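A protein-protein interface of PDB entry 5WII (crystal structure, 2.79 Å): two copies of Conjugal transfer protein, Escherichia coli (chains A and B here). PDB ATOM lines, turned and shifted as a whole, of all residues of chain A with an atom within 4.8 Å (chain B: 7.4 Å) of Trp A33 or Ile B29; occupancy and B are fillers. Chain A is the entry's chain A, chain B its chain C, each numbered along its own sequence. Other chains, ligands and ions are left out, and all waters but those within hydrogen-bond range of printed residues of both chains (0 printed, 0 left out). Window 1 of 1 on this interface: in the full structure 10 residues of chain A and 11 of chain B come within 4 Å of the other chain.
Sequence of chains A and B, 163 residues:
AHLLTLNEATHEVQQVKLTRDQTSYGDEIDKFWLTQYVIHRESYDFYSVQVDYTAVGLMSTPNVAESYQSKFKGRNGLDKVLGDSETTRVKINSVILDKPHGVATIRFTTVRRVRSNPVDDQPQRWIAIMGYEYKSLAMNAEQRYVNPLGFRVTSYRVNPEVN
The side-chain hydroxyl of Thr A35 lies within hydrogen-bond range of the backbone carbonyl oxygen of Phe A32.
O of Phe B32 is in hydrogen-bond range of OG1 of Thr B35 (2.9 Å).
Of the 16 printed residues of chain A, 6 touch a printed residue of chain B.
Printed residues of chain A that touch a printed residue of chain B: Ile A29, Phe A32, Trp A33, Gln A36, Pro A148 and Leu A149.
Printed residues of chain B that touch a printed residue of chain A: Tyr B25, Glu B28, Ile B29, Phe B32, Trp B33 and Leu B149.
Hydrophobic or aromatic side chains of chain B that line the printed part of chain A: Tyr B25, Ile B29, Phe B32, Trp B33 and Leu B149.
Printed residues of chain B within 4 Å of Phe A32: Glu B28 (3.6 Å), Ile B29 (3.9 Å) and Phe B32 (3.3 Å).
Trp A33 touches just one residue of chain B: Ile B29 (3.3 Å).
Asp B27 touches none of the printed residues of chain A.
Printed residues of chain A within 4 Å of Glu B28: Phe A32 (3.6 Å) and Gln A36 (3.8 Å).
Printed residues of chain A within 4 Å of Ile B29: Phe A32 (3.9 Å), Trp A33 (3.3 Å) and Pro A148 (3.8 Å).
The nearest residue of chain A that does not touch Ile B29 is Val A146 (4.3 Å).
The nearest printed residue of chain A that does not touch Leu B149 is Pro A148 (4.5 Å).
Phe B32 touches Ile A29 (CE2 to CD1, 3.6 Å).
CD1 of Ile A29 touches CH2 of Trp B33, 3.6 Å away.
Phe A32 touches Glu B28 (CZ to O, 3.6 Å).
Ile B29 touches Phe A32.
Phe B32 touches Phe A32 (CD1 to CD1, 3.3 Å).
CD1 of Ile B29 touches CH2 of Trp A33 (3.3 Å).
Glu B28 touches Gln A36 (CB to NE2, 3.8 Å).
CB of Pro A148 touches CE2 of Tyr B25 (3.5 Å).
Ile B29 touches Pro A148.
Leu A149 touches Leu B149.
Ile A29 touches Phe B32, and with the chains exchanged Phe A32 touches Ile B29.
Ile A29 touches Trp B33, and with the chains exchanged Trp A33 touches Ile B29.
Phe B32 touches its own counterpart, Phe A32.
Leu B149 touches its own counterpart, Leu A149.
Of the 10 pairs that touch across the chains among the printed residues, 6 have their exchanged pair printed and touching as well.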
ATOM      1  N   ILE A  29      27.291   8.183  17.190  1.00  0.00           N
ATOM      2  CA  ILE A  29      26.538   8.631  18.356  1.00  0.00           C
ATOM      3  C   ILE A  29      25.293   9.392  17.916  1.00  0.00           C
ATOM      4  O   ILE A  29      24.183   9.088  18.354  1.00  0.00           O
ATOM      5  CB  ILE A  29      27.399   9.529  19.273  1.00  0.00           C
ATOM      6  CG1 ILE A  29      28.564   8.729  19.863  1.00  0.00           C
ATOM      7  CG2 ILE A  29      26.554  10.150  20.388  1.00  0.00           C
ATOM      8  CD1 ILE A  29      28.150   7.614  20.815  1.00  0.00           C
ATOM      9  N   ASP A  30      25.486  10.387  17.057  1.00  0.00           N
ATOM     10  CA  ASP A  30      24.378  11.170  16.523  1.00  0.00           C
ATOM     11  C   ASP A  30      23.354  10.262  15.852  1.00  0.00           C
ATOM     12  O   ASP A  30      22.150  10.437  16.022  1.00  0.00           O
ATOM     13  CB  ASP A  30      24.891  12.210  15.526  1.00  0.00           C
ATOM     14  CG  ASP A  30      25.839  13.207  16.158  1.00  0.00           C
ATOM     15  OD1 ASP A  30      26.347  12.925  17.264  1.00  0.00           O
ATOM     16  OD2 ASP A  30      26.081  14.268  15.548  1.00  0.00           O
ATOM     17  N   LYS A  31      23.851   9.288  15.098  1.00  0.00           N
ATOM     18  CA  LYS A  31      23.002   8.325  14.405  1.00  0.00           C
ATOM     19  C   LYS A  31      22.129   7.550  15.386  1.00  0.00           C
ATOM     20  O   LYS A  31      20.970   7.251  15.100  1.00  0.00           O
ATOM     21  CB  LYS A  31      23.867   7.360  13.589  1.00  0.00           C
ATOM     22  CG  LYS A  31      23.120   6.199  12.956  1.00  0.00           C
ATOM     23  CD  LYS A  31      24.070   5.336  12.141  1.00  0.00           C
ATOM     24  CE  LYS A  31      23.370   4.121  11.560  1.00  0.00           C
ATOM     25  NZ  LYS A  31      24.310   3.257  10.792  1.00  0.00           N
ATOM     26  N   PHE A  32      22.689   7.233  16.548  1.00  0.00           N
ATOM     27  CA  PHE A  32      21.987   6.432  17.544  1.00  0.00           C
ATOM     28  C   PHE A  32      20.796   7.172  18.148  1.00  0.00           C
ATOM     29  O   PHE A  32      19.670   6.677  18.119  1.00  0.00           O
ATOM     30  CB  PHE A  32      22.950   6.012  18.656  1.00  0.00           C
ATOM     31  CG  PHE A  32      22.274   5.362  19.827  1.00  0.00           C
ATOM     32  CD1 PHE A  32      21.912   4.026  19.781  1.00  0.00           C
ATOM     33  CD2 PHE A  32      22.003   6.084  20.976  1.00  0.00           C
ATOM     34  CE1 PHE A  32      21.290   3.425  20.858  1.00  0.00           C
ATOM     35  CE2 PHE A  32      21.383   5.489  22.056  1.00  0.00           C
ATOM     36  CZ  PHE A  32      21.026   4.158  21.998  1.00  0.00           C
ATOM     37  N   TRP A  33      21.038   8.371  18.664  1.00  0.00           N
ATOM     38  CA  TRP A  33      20.004   9.124  19.348  1.00  0.00           C
ATOM     39  C   TRP A  33      18.862   9.436  18.426  1.00  0.00           C
ATOM     40  O   TRP A  33      17.681   9.382  18.831  1.00  0.00           O
ATOM     41  CB  TRP A  33      20.579  10.417  19.914  1.00  0.00           C
ATOM     42  CG  TRP A  33      21.618  10.195  20.987  1.00  0.00           C
ATOM     43  CD1 TRP A  33      22.983  10.459  20.917  1.00  0.00           C
ATOM     44  CD2 TRP A  33      21.405   9.652  22.337  1.00  0.00           C
ATOM     45  NE1 TRP A  33      23.608  10.127  22.093  1.00  0.00           N
ATOM     46  CE2 TRP A  33      22.720   9.638  22.985  1.00  0.00           C
ATOM     47  CE3 TRP A  33      20.304   9.195  23.044  1.00  0.00           C
ATOM     48  CZ2 TRP A  33      22.893   9.183  24.280  1.00  0.00           C
ATOM     49  CZ3 TRP A  33      20.493   8.739  24.350  1.00  0.00           C
ATOM     50  CH2 TRP A  33      21.757   8.734  24.951  1.00  0.00           C
ATOM     51  N   LEU A  34      19.185   9.768  17.181  1.00  0.00           N
ATOM     52  CA  LEU A  34      18.175  10.131  16.195  1.00  0.00           C
ATOM     53  C   LEU A  34      17.265   8.950  15.883  1.00  0.00           C
ATOM     54  O   LEU A  34      16.046   9.094  15.837  1.00  0.00           O
ATOM     55  CB  LEU A  34      18.840  10.637  14.917  1.00  0.00           C
ATOM     56  CG  LEU A  34      19.614  11.948  15.054  1.00  0.00           C
ATOM     57  CD1 LEU A  34      20.529  12.148  13.858  1.00  0.00           C
ATOM     58  CD2 LEU A  34      18.664  13.122  15.199  1.00  0.00           C
ATOM     59  N   THR A  35      17.864   7.783  15.665  1.00  0.00           N
ATOM     60  CA  THR A  35      17.099   6.568  15.414  1.00  0.00           C
ATOM     61  C   THR A  35      16.216   6.240  16.614  1.00  0.00           C
ATOM     62  O   THR A  35      15.059   5.847  16.458  1.00  0.00           O
ATOM     63  CB  THR A  35      18.019   5.368  15.110  1.00  0.00           C
ATOM     64  OG1 THR A  35      19.059   5.293  16.094  1.00  0.00           O
ATOM     65  CG2 THR A  35      18.642   5.508  13.732  1.00  0.00           C
ATOM     66  N   GLN A  36      16.768   6.413  17.810  1.00  0.00           N
ATOM     67  CA  GLN A  36      16.019   6.189  19.042  1.00  0.00           C
ATOM     68  C   GLN A  36      14.854   7.165  19.159  1.00  0.00           C
ATOM     69  O   GLN A  36      13.797   6.826  19.692  1.00  0.00           O
ATOM     70  CB  GLN A  36      16.939   6.322  20.256  1.00  0.00           C
ATOM     71  CG  GLN A  36      17.919   5.173  20.414  1.00  0.00           C
ATOM     72  CD  GLN A  36      17.234   3.880  20.804  1.00  0.00           C
ATOM     73  OE1 GLN A  36      17.306   2.883  20.084  1.00  0.00           O
ATOM     74  NE2 GLN A  36      16.566   3.887  21.952  1.00  0.00           N
ATOM     75  N   TYR A  37      15.051   8.376  18.653  1.00  0.00           N
ATOM     76  CA  TYR A  37      14.033   9.413  18.725  1.00  0.00           C
ATOM     77  C   TYR A  37      12.831   9.065  17.849  1.00  0.00           C
ATOM     78  O   TYR A  37      11.687   9.167  18.288  1.00  0.00           O
ATOM     79  CB  TYR A  37      14.623  10.762  18.310  1.00  0.00           C
ATOM     80  CG  TYR A  37      13.665  11.924  18.429  1.00  0.00           C
ATOM     81  CD1 TYR A  37      13.537  12.626  19.619  1.00  0.00           C
ATOM     82  CD2 TYR A  37      12.897  12.328  17.346  1.00  0.00           C
ATOM     83  CE1 TYR A  37      12.666  13.693  19.729  1.00  0.00           C
ATOM     84  CE2 TYR A  37      12.025  13.391  17.447  1.00  0.00           C
ATOM     85  CZ  TYR A  37      11.913  14.072  18.638  1.00  0.00           C
ATOM     86  OH  TYR A  37      11.042  15.133  18.732  1.00  0.00           O
ATOM     87  N   MET A  59      14.215  14.849  24.830  1.00  0.00           N
ATOM     88  CA  MET A  59      14.896  14.870  23.539  1.00  0.00           C
ATOM     89  C   MET A  59      14.304  15.900  22.582  1.00  0.00           C
ATOM     90  O   MET A  59      14.452  15.778  21.366  1.00  0.00           O
ATOM     91  CB  MET A  59      14.840  13.486  22.887  1.00  0.00           C
ATOM     92  CG  MET A  59      15.656  12.424  23.597  1.00  0.00           C
ATOM     93  SD  MET A  59      15.441  10.798  22.855  1.00  0.00           S
ATOM     94  CE  MET A  59      16.777   9.888  23.619  1.00  0.00           C
ATOM     95  N   TYR A 134      23.177  19.170  21.274  1.00  0.00           N
ATOM     96  CA  TYR A 134      23.305  18.775  22.670  1.00  0.00           C
ATOM     97  C   TYR A 134      23.453  20.060  23.474  1.00  0.00           C
ATOM     98  O   TYR A 134      24.022  21.031  22.978  1.00  0.00           O
ATOM     99  CB  TYR A 134      24.498  17.839  22.877  1.00  0.00           C
ATOM    100  CG  TYR A 134      24.475  16.598  22.002  1.00  0.00           C
ATOM    101  CD1 TYR A 134      24.576  16.690  20.619  1.00  0.00           C
ATOM    102  CD2 TYR A 134      24.367  15.332  22.562  1.00  0.00           C
ATOM    103  CE1 TYR A 134      24.559  15.565  19.820  1.00  0.00           C
ATOM    104  CE2 TYR A 134      24.351  14.198  21.768  1.00  0.00           C
ATOM    105  CZ  TYR A 134      24.447  14.322  20.397  1.00  0.00           C
ATOM    106  OH  TYR A 134      24.432  13.202  19.599  1.00  0.00           O
ATOM    107  N   VAL A 146      17.637   8.367  30.645  1.00  0.00           N
ATOM    108  CA  VAL A 146      17.079   8.323  29.297  1.00  0.00           C
ATOM    109  C   VAL A 146      17.926   9.147  28.328  1.00  0.00           C
ATOM    110  O   VAL A 146      18.151   8.740  27.188  1.00  0.00           O
ATOM    111  CB  VAL A 146      15.627   8.842  29.279  1.00  0.00           C
ATOM    112  CG1 VAL A 146      15.073   8.866  27.860  1.00  0.00           C
ATOM    113  CG2 VAL A 146      14.748   7.981  30.176  1.00  0.00           C
ATOM    114  N   ASN A 147      18.361  10.320  28.791  1.00  0.00           N
ATOM    115  CA  ASN A 147      19.153  11.250  27.984  1.00  0.00           C
ATOM    116  C   ASN A 147      20.396  11.790  28.706  1.00  0.00           C
ATOM    117  O   ASN A 147      20.405  12.929  29.172  1.00  0.00           O
ATOM    118  CB  ASN A 147      18.281  12.421  27.526  1.00  0.00           C
ATOM    119  CG  ASN A 147      18.938  13.247  26.437  1.00  0.00           C
ATOM    120  OD1 ASN A 147      19.829  14.052  26.707  1.00  0.00           O
ATOM    121  ND2 ASN A 147      18.500  13.051  25.199  1.00  0.00           N
ATOM    122  N   PRO A 148      21.437  10.968  28.795  1.00  0.00           N
ATOM    123  CA  PRO A 148      22.689  11.331  29.470  1.00  0.00           C
ATOM    124  C   PRO A 148      23.421  12.538  28.887  1.00  0.00           C
ATOM    125  O   PRO A 148      24.116  13.223  29.634  1.00  0.00           O
ATOM    126  CB  PRO A 148      23.556  10.079  29.295  1.00  0.00           C
ATOM    127  CG  PRO A 148      22.610   8.973  29.073  1.00  0.00           C
ATOM    128  CD  PRO A 148      21.446   9.563  28.351  1.00  0.00           C
ATOM    129  N   LEU A 149      23.285  12.786  27.587  1.00  0.00           N
ATOM    130  CA  LEU A 149      24.131  13.774  26.919  1.00  0.00           C
ATOM    131  C   LEU A 149      23.412  15.077  26.581  1.00  0.00           C
ATOM    132  O   LEU A 149      24.006  15.980  25.994  1.00  0.00           O
ATOM    133  CB  LEU A 149      24.720  13.170  25.643  1.00  0.00           C
ATOM    134  CG  LEU A 149      25.609  11.941  25.857  1.00  0.00           C
ATOM    135  CD1 LEU A 149      25.995  11.338  24.520  1.00  0.00           C
ATOM    136  CD2 LEU A 149      26.852  12.296  26.663  1.00  0.00           C
ATOM    137  N   PHE A 151      21.000  15.429  24.508  1.00  0.00           N
ATOM    138  CA  PHE A 151      20.560  15.430  23.119  1.00  0.00           C
ATOM    139  C   PHE A 151      19.106  15.864  23.040  1.00  0.00           C
ATOM    140  O   PHE A 151      18.250  15.293  23.714  1.00  0.00           O
ATOM    141  CB  PHE A 151      20.727  14.046  22.487  1.00  0.00           C
ATOM    142  CG  PHE A 151      20.002  13.886  21.178  1.00  0.00           C
ATOM    143  CD1 PHE A 151      20.561  14.346  19.998  1.00  0.00           C
ATOM    144  CD2 PHE A 151      18.760  13.276  21.131  1.00  0.00           C
ATOM    145  CE1 PHE A 151      19.894  14.200  18.796  1.00  0.00           C
ATOM    146  CE2 PHE A 151      18.089  13.127  19.932  1.00  0.00           C
ATOM    147  CZ  PHE A 151      18.657  13.590  18.764  1.00  0.00           C
ATOM    148  N   TYR B  25      22.425   4.099  33.331  1.00  0.00           N
ATOM    149  CA  TYR B  25      22.418   4.871  32.087  1.00  0.00           C
ATOM    150  C   TYR B  25      21.367   4.444  31.063  1.00  0.00           C
ATOM    151  O   TYR B  25      21.095   5.183  30.118  1.00  0.00           O
ATOM    152  CB  TYR B  25      23.801   4.807  31.439  1.00  0.00           C
ATOM    153  CG  TYR B  25      24.642   6.010  31.767  1.00  0.00           C
ATOM    154  CD1 TYR B  25      25.075   6.238  33.064  1.00  0.00           C
ATOM    155  CD2 TYR B  25      24.979   6.934  30.789  1.00  0.00           C
ATOM    156  CE1 TYR B  25      25.835   7.344  33.378  1.00  0.00           C
ATOM    157  CE2 TYR B  25      25.741   8.045  31.090  1.00  0.00           C
ATOM    158  CZ  TYR B  25      26.166   8.245  32.390  1.00  0.00           C
ATOM    159  OH  TYR B  25      26.924   9.348  32.708  1.00  0.00           O
ATOM    160  N   GLY B  26      20.782   3.263  31.242  1.00  0.00           N
ATOM    161  CA  GLY B  26      19.754   2.782  30.335  1.00  0.00           C
ATOM    162  C   GLY B  26      20.185   1.571  29.533  1.00  0.00           C
ATOM    163  O   GLY B  26      21.364   1.403  29.225  1.00  0.00           O
ATOM    164  N   ASP B  27      19.217   0.734  29.181  1.00  0.00           N
ATOM    165  CA  ASP B  27      19.500  -0.539  28.534  1.00  0.00           C
ATOM    166  C   ASP B  27      19.919  -0.390  27.074  1.00  0.00           C
ATOM    167  O   ASP B  27      20.916  -0.974  26.648  1.00  0.00           O
ATOM    168  CB  ASP B  27      18.276  -1.447  28.627  1.00  0.00           C
ATOM    169  CG  ASP B  27      17.902  -1.764  30.058  1.00  0.00           C
ATOM    170  OD1 ASP B  27      18.272  -0.976  30.955  1.00  0.00           O
ATOM    171  OD2 ASP B  27      17.240  -2.797  30.288  1.00  0.00           O
ATOM    172  N   GLU B  28      19.163   0.390  26.308  1.00  0.00           N
ATOM    173  CA  GLU B  28      19.410   0.507  24.873  1.00  0.00           C
ATOM    174  C   GLU B  28      20.753   1.180  24.601  1.00  0.00           C
ATOM    175  O   GLU B  28      21.364   0.962  23.553  1.00  0.00           O
ATOM    176  CB  GLU B  28      18.288   1.287  24.184  1.00  0.00           C
ATOM    177  CG  GLU B  28      16.902   0.663  24.328  1.00  0.00           C
ATOM    178  CD  GLU B  28      16.249   0.940  25.675  1.00  0.00           C
ATOM    179  OE1 GLU B  28      16.801   1.734  26.466  1.00  0.00           O
ATOM    180  OE2 GLU B  28      15.178   0.355  25.943  1.00  0.00           O
ATOM    181  N   ILE B  29      21.211   1.995  25.546  1.00  0.00           N
ATOM    182  CA  ILE B  29      22.501   2.662  25.421  1.00  0.00           C
ATOM    183  C   ILE B  29      23.634   1.679  25.695  1.00  0.00           C
ATOM    184  O   ILE B  29      24.618   1.641  24.962  1.00  0.00           O
ATOM    185  CB  ILE B  29      22.605   3.866  26.377  1.00  0.00           C
ATOM    186  CG1 ILE B  29      21.634   4.963  25.933  1.00  0.00           C
ATOM    187  CG2 ILE B  29      24.030   4.420  26.409  1.00  0.00           C
ATOM    188  CD1 ILE B  29      21.472   6.092  26.924  1.00  0.00           C
ATOM    189  N   ASP B  30      23.497   0.890  26.755  1.00  0.00           N
ATOM    190  CA  ASP B  30      24.491  -0.129  27.069  1.00  0.00           C
ATOM    191  C   ASP B  30      24.597  -1.112  25.911  1.00  0.00           C
ATOM    192  O   ASP B  30      25.688  -1.553  25.554  1.00  0.00           O
ATOM    193  CB  ASP B  30      24.133  -0.861  28.363  1.00  0.00           C
ATOM    194  CG  ASP B  30      24.254   0.027  29.587  1.00  0.00           C
ATOM    195  OD1 ASP B  30      24.250   1.264  29.429  1.00  0.00           O
ATOM    196  OD2 ASP B  30      24.350  -0.515  30.708  1.00  0.00           O
ATOM    197  N   LYS B  31      23.451  -1.442  25.322  1.00  0.00           N
ATOM    198  CA  LYS B  31      23.407  -2.306  24.150  1.00  0.00           C
ATOM    199  C   LYS B  31      24.216  -1.705  23.005  1.00  0.00           C
ATOM    200  O   LYS B  31      24.853  -2.424  22.237  1.00  0.00           O
ATOM    201  CB  LYS B  31      21.955  -2.536  23.716  1.00  0.00           C
ATOM    202  CG  LYS B  31      21.792  -3.270  22.389  1.00  0.00           C
ATOM    203  CD  LYS B  31      21.644  -2.307  21.215  1.00  0.00           C
ATOM    204  CE  LYS B  31      21.467  -3.050  19.902  1.00  0.00           C
ATOM    205  NZ  LYS B  31      21.561  -2.134  18.731  1.00  0.00           N
ATOM    206  N   PHE B  32      24.186  -0.380  22.898  1.00  0.00           N
ATOM    207  CA  PHE B  32      24.853   0.314  21.802  1.00  0.00           C
ATOM    208  C   PHE B  32      26.374   0.267  21.927  1.00  0.00           C
ATOM    209  O   PHE B  32      27.057  -0.181  21.009  1.00  0.00           O
ATOM    210  CB  PHE B  32      24.385   1.770  21.733  1.00  0.00           C
ATOM    211  CG  PHE B  32      25.200   2.624  20.807  1.00  0.00           C
ATOM    212  CD1 PHE B  32      24.934   2.644  19.449  1.00  0.00           C
ATOM    213  CD2 PHE B  32      26.230   3.411  21.295  1.00  0.00           C
ATOM    214  CE1 PHE B  32      25.682   3.430  18.594  1.00  0.00           C
ATOM    215  CE2 PHE B  32      26.981   4.198  20.445  1.00  0.00           C
ATOM    216  CZ  PHE B  32      26.706   4.209  19.092  1.00  0.00           C
ATOM    217  N   TRP B  33      26.899   0.659  23.080  1.00  0.00           N
ATOM    218  CA  TRP B  33      28.333   0.773  23.248  1.00  0.00           C
ATOM    219  C   TRP B  33      28.986  -0.555  23.014  1.00  0.00           C
ATOM    220  O   TRP B  33      30.097  -0.633  22.446  1.00  0.00           O
ATOM    221  CB  TRP B  33      28.664   1.278  24.646  1.00  0.00           C
ATOM    222  CG  TRP B  33      28.251   2.712  24.883  1.00  0.00           C
ATOM    223  CD1 TRP B  33      27.138   3.172  25.580  1.00  0.00           C
ATOM    224  CD2 TRP B  33      28.942   3.927  24.425  1.00  0.00           C
ATOM    225  NE1 TRP B  33      27.094   4.544  25.584  1.00  0.00           N
ATOM    226  CE2 TRP B  33      28.146   5.057  24.909  1.00  0.00           C
ATOM    227  CE3 TRP B  33      30.091   4.180  23.693  1.00  0.00           C
ATOM    228  CZ2 TRP B  33      28.507   6.369  24.658  1.00  0.00           C
ATOM    229  CZ3 TRP B  33      30.445   5.508  23.446  1.00  0.00           C
ATOM    230  CH2 TRP B  33      29.670   6.574  23.918  1.00  0.00           C
ATOM    231  N   LEU B  34      28.322  -1.617  23.453  1.00  0.00           N
ATOM    232  CA  LEU B  34      28.878  -2.964  23.388  1.00  0.00           C
ATOM    233  C   LEU B  34      28.986  -3.476  21.957  1.00  0.00           C
ATOM    234  O   LEU B  34      30.051  -3.916  21.529  1.00  0.00           O
ATOM    235  CB  LEU B  34      28.025  -3.921  24.215  1.00  0.00           C
ATOM    236  CG  LEU B  34      28.011  -3.641  25.716  1.00  0.00           C
ATOM    237  CD1 LEU B  34      26.842  -4.358  26.360  1.00  0.00           C
ATOM    238  CD2 LEU B  34      29.322  -4.068  26.356  1.00  0.00           C
ATOM    239  N   THR B  35      27.877  -3.427  21.224  1.00  0.00           N
ATOM    240  CA  THR B  35      27.844  -3.919  19.852  1.00  0.00           C
ATOM    241  C   THR B  35      28.877  -3.211  18.982  1.00  0.00           C
ATOM    242  O   THR B  35      29.611  -3.851  18.230  1.00  0.00           O
ATOM    243  CB  THR B  35      26.452  -3.738  19.221  1.00  0.00           C
ATOM    244  OG1 THR B  35      25.979  -2.408  19.471  1.00  0.00           O
ATOM    245  CG2 THR B  35      25.471  -4.739  19.800  1.00  0.00           C
ATOM    246  N   LEU B  97      21.459  -8.158  28.253  1.00  0.00           N
ATOM    247  CA  LEU B  97      22.136  -7.417  29.315  1.00  0.00           C
ATOM    248  C   LEU B  97      21.999  -8.058  30.693  1.00  0.00           C
ATOM    249  O   LEU B  97      21.011  -8.731  30.993  1.00  0.00           O
ATOM    250  CB  LEU B  97      21.597  -5.985  29.385  1.00  0.00           C
ATOM    251  CG  LEU B  97      21.916  -5.045  28.223  1.00  0.00           C
ATOM    252  CD1 LEU B  97      21.240  -3.705  28.450  1.00  0.00           C
ATOM    253  CD2 LEU B  97      23.417  -4.859  28.056  1.00  0.00           C
ATOM    254  N   TYR B 134      31.492   2.508  34.076  1.00  0.00           N
ATOM    255  CA  TYR B 134      31.784   3.922  33.861  1.00  0.00           C
ATOM    256  C   TYR B 134      32.608   4.458  35.028  1.00  0.00           C
ATOM    257  O   TYR B 134      32.335   4.135  36.185  1.00  0.00           O
ATOM    258  CB  TYR B 134      30.492   4.735  33.717  1.00  0.00           C
ATOM    259  CG  TYR B 134      29.543   4.229  32.651  1.00  0.00           C
ATOM    260  CD1 TYR B 134      28.826   3.053  32.831  1.00  0.00           C
ATOM    261  CD2 TYR B 134      29.350   4.938  31.473  1.00  0.00           C
ATOM    262  CE1 TYR B 134      27.956   2.588  31.863  1.00  0.00           C
ATOM    263  CE2 TYR B 134      28.481   4.482  30.499  1.00  0.00           C
ATOM    264  CZ  TYR B 134      27.786   3.308  30.700  1.00  0.00           C
ATOM    265  OH  TYR B 134      26.918   2.848  29.735  1.00  0.00           O
ATOM    266  N   LEU B 149      31.398   9.445  28.146  1.00  0.00           N
ATOM    267  CA  LEU B 149      30.895   8.913  29.410  1.00  0.00           C
ATOM    268  C   LEU B 149      31.963   8.230  30.262  1.00  0.00           C
ATOM    269  O   LEU B 149      31.692   7.824  31.392  1.00  0.00           O
ATOM    270  CB  LEU B 149      29.762   7.924  29.133  1.00  0.00           C
ATOM    271  CG  LEU B 149      28.619   8.463  28.270  1.00  0.00           C
ATOM    272  CD1 LEU B 149      27.576   7.384  28.036  1.00  0.00           C
ATOM    273  CD2 LEU B 149      27.993   9.692  28.911  1.00  0.00           C
ATOM    274  N   PHE B 151      33.093   5.433  29.599  1.00  0.00           N
ATOM    275  CA  PHE B 151      32.773   4.014  29.497  1.00  0.00           C
ATOM    276  C   PHE B 151      34.032   3.218  29.166  1.00  0.00           C
ATOM    277  O   PHE B 151      34.716   3.511  28.183  1.00  0.00           O
ATOM    278  CB  PHE B 151      31.689   3.793  28.434  1.00  0.00           C
ATOM    279  CG  PHE B 151      31.573   2.371  27.962  1.00  0.00           C
ATOM    280  CD1 PHE B 151      30.757   1.472  28.626  1.00  0.00           C
ATOM    281  CD2 PHE B 151      32.266   1.938  26.842  1.00  0.00           C
ATOM    282  CE1 PHE B 151      30.643   0.166  28.190  1.00  0.00           C
ATOM    283  CE2 PHE B 151      32.157   0.633  26.404  1.00  0.00           C
ATOM    284  CZ  PHE B 151      31.344  -0.253  27.077  1.00  0.00           C
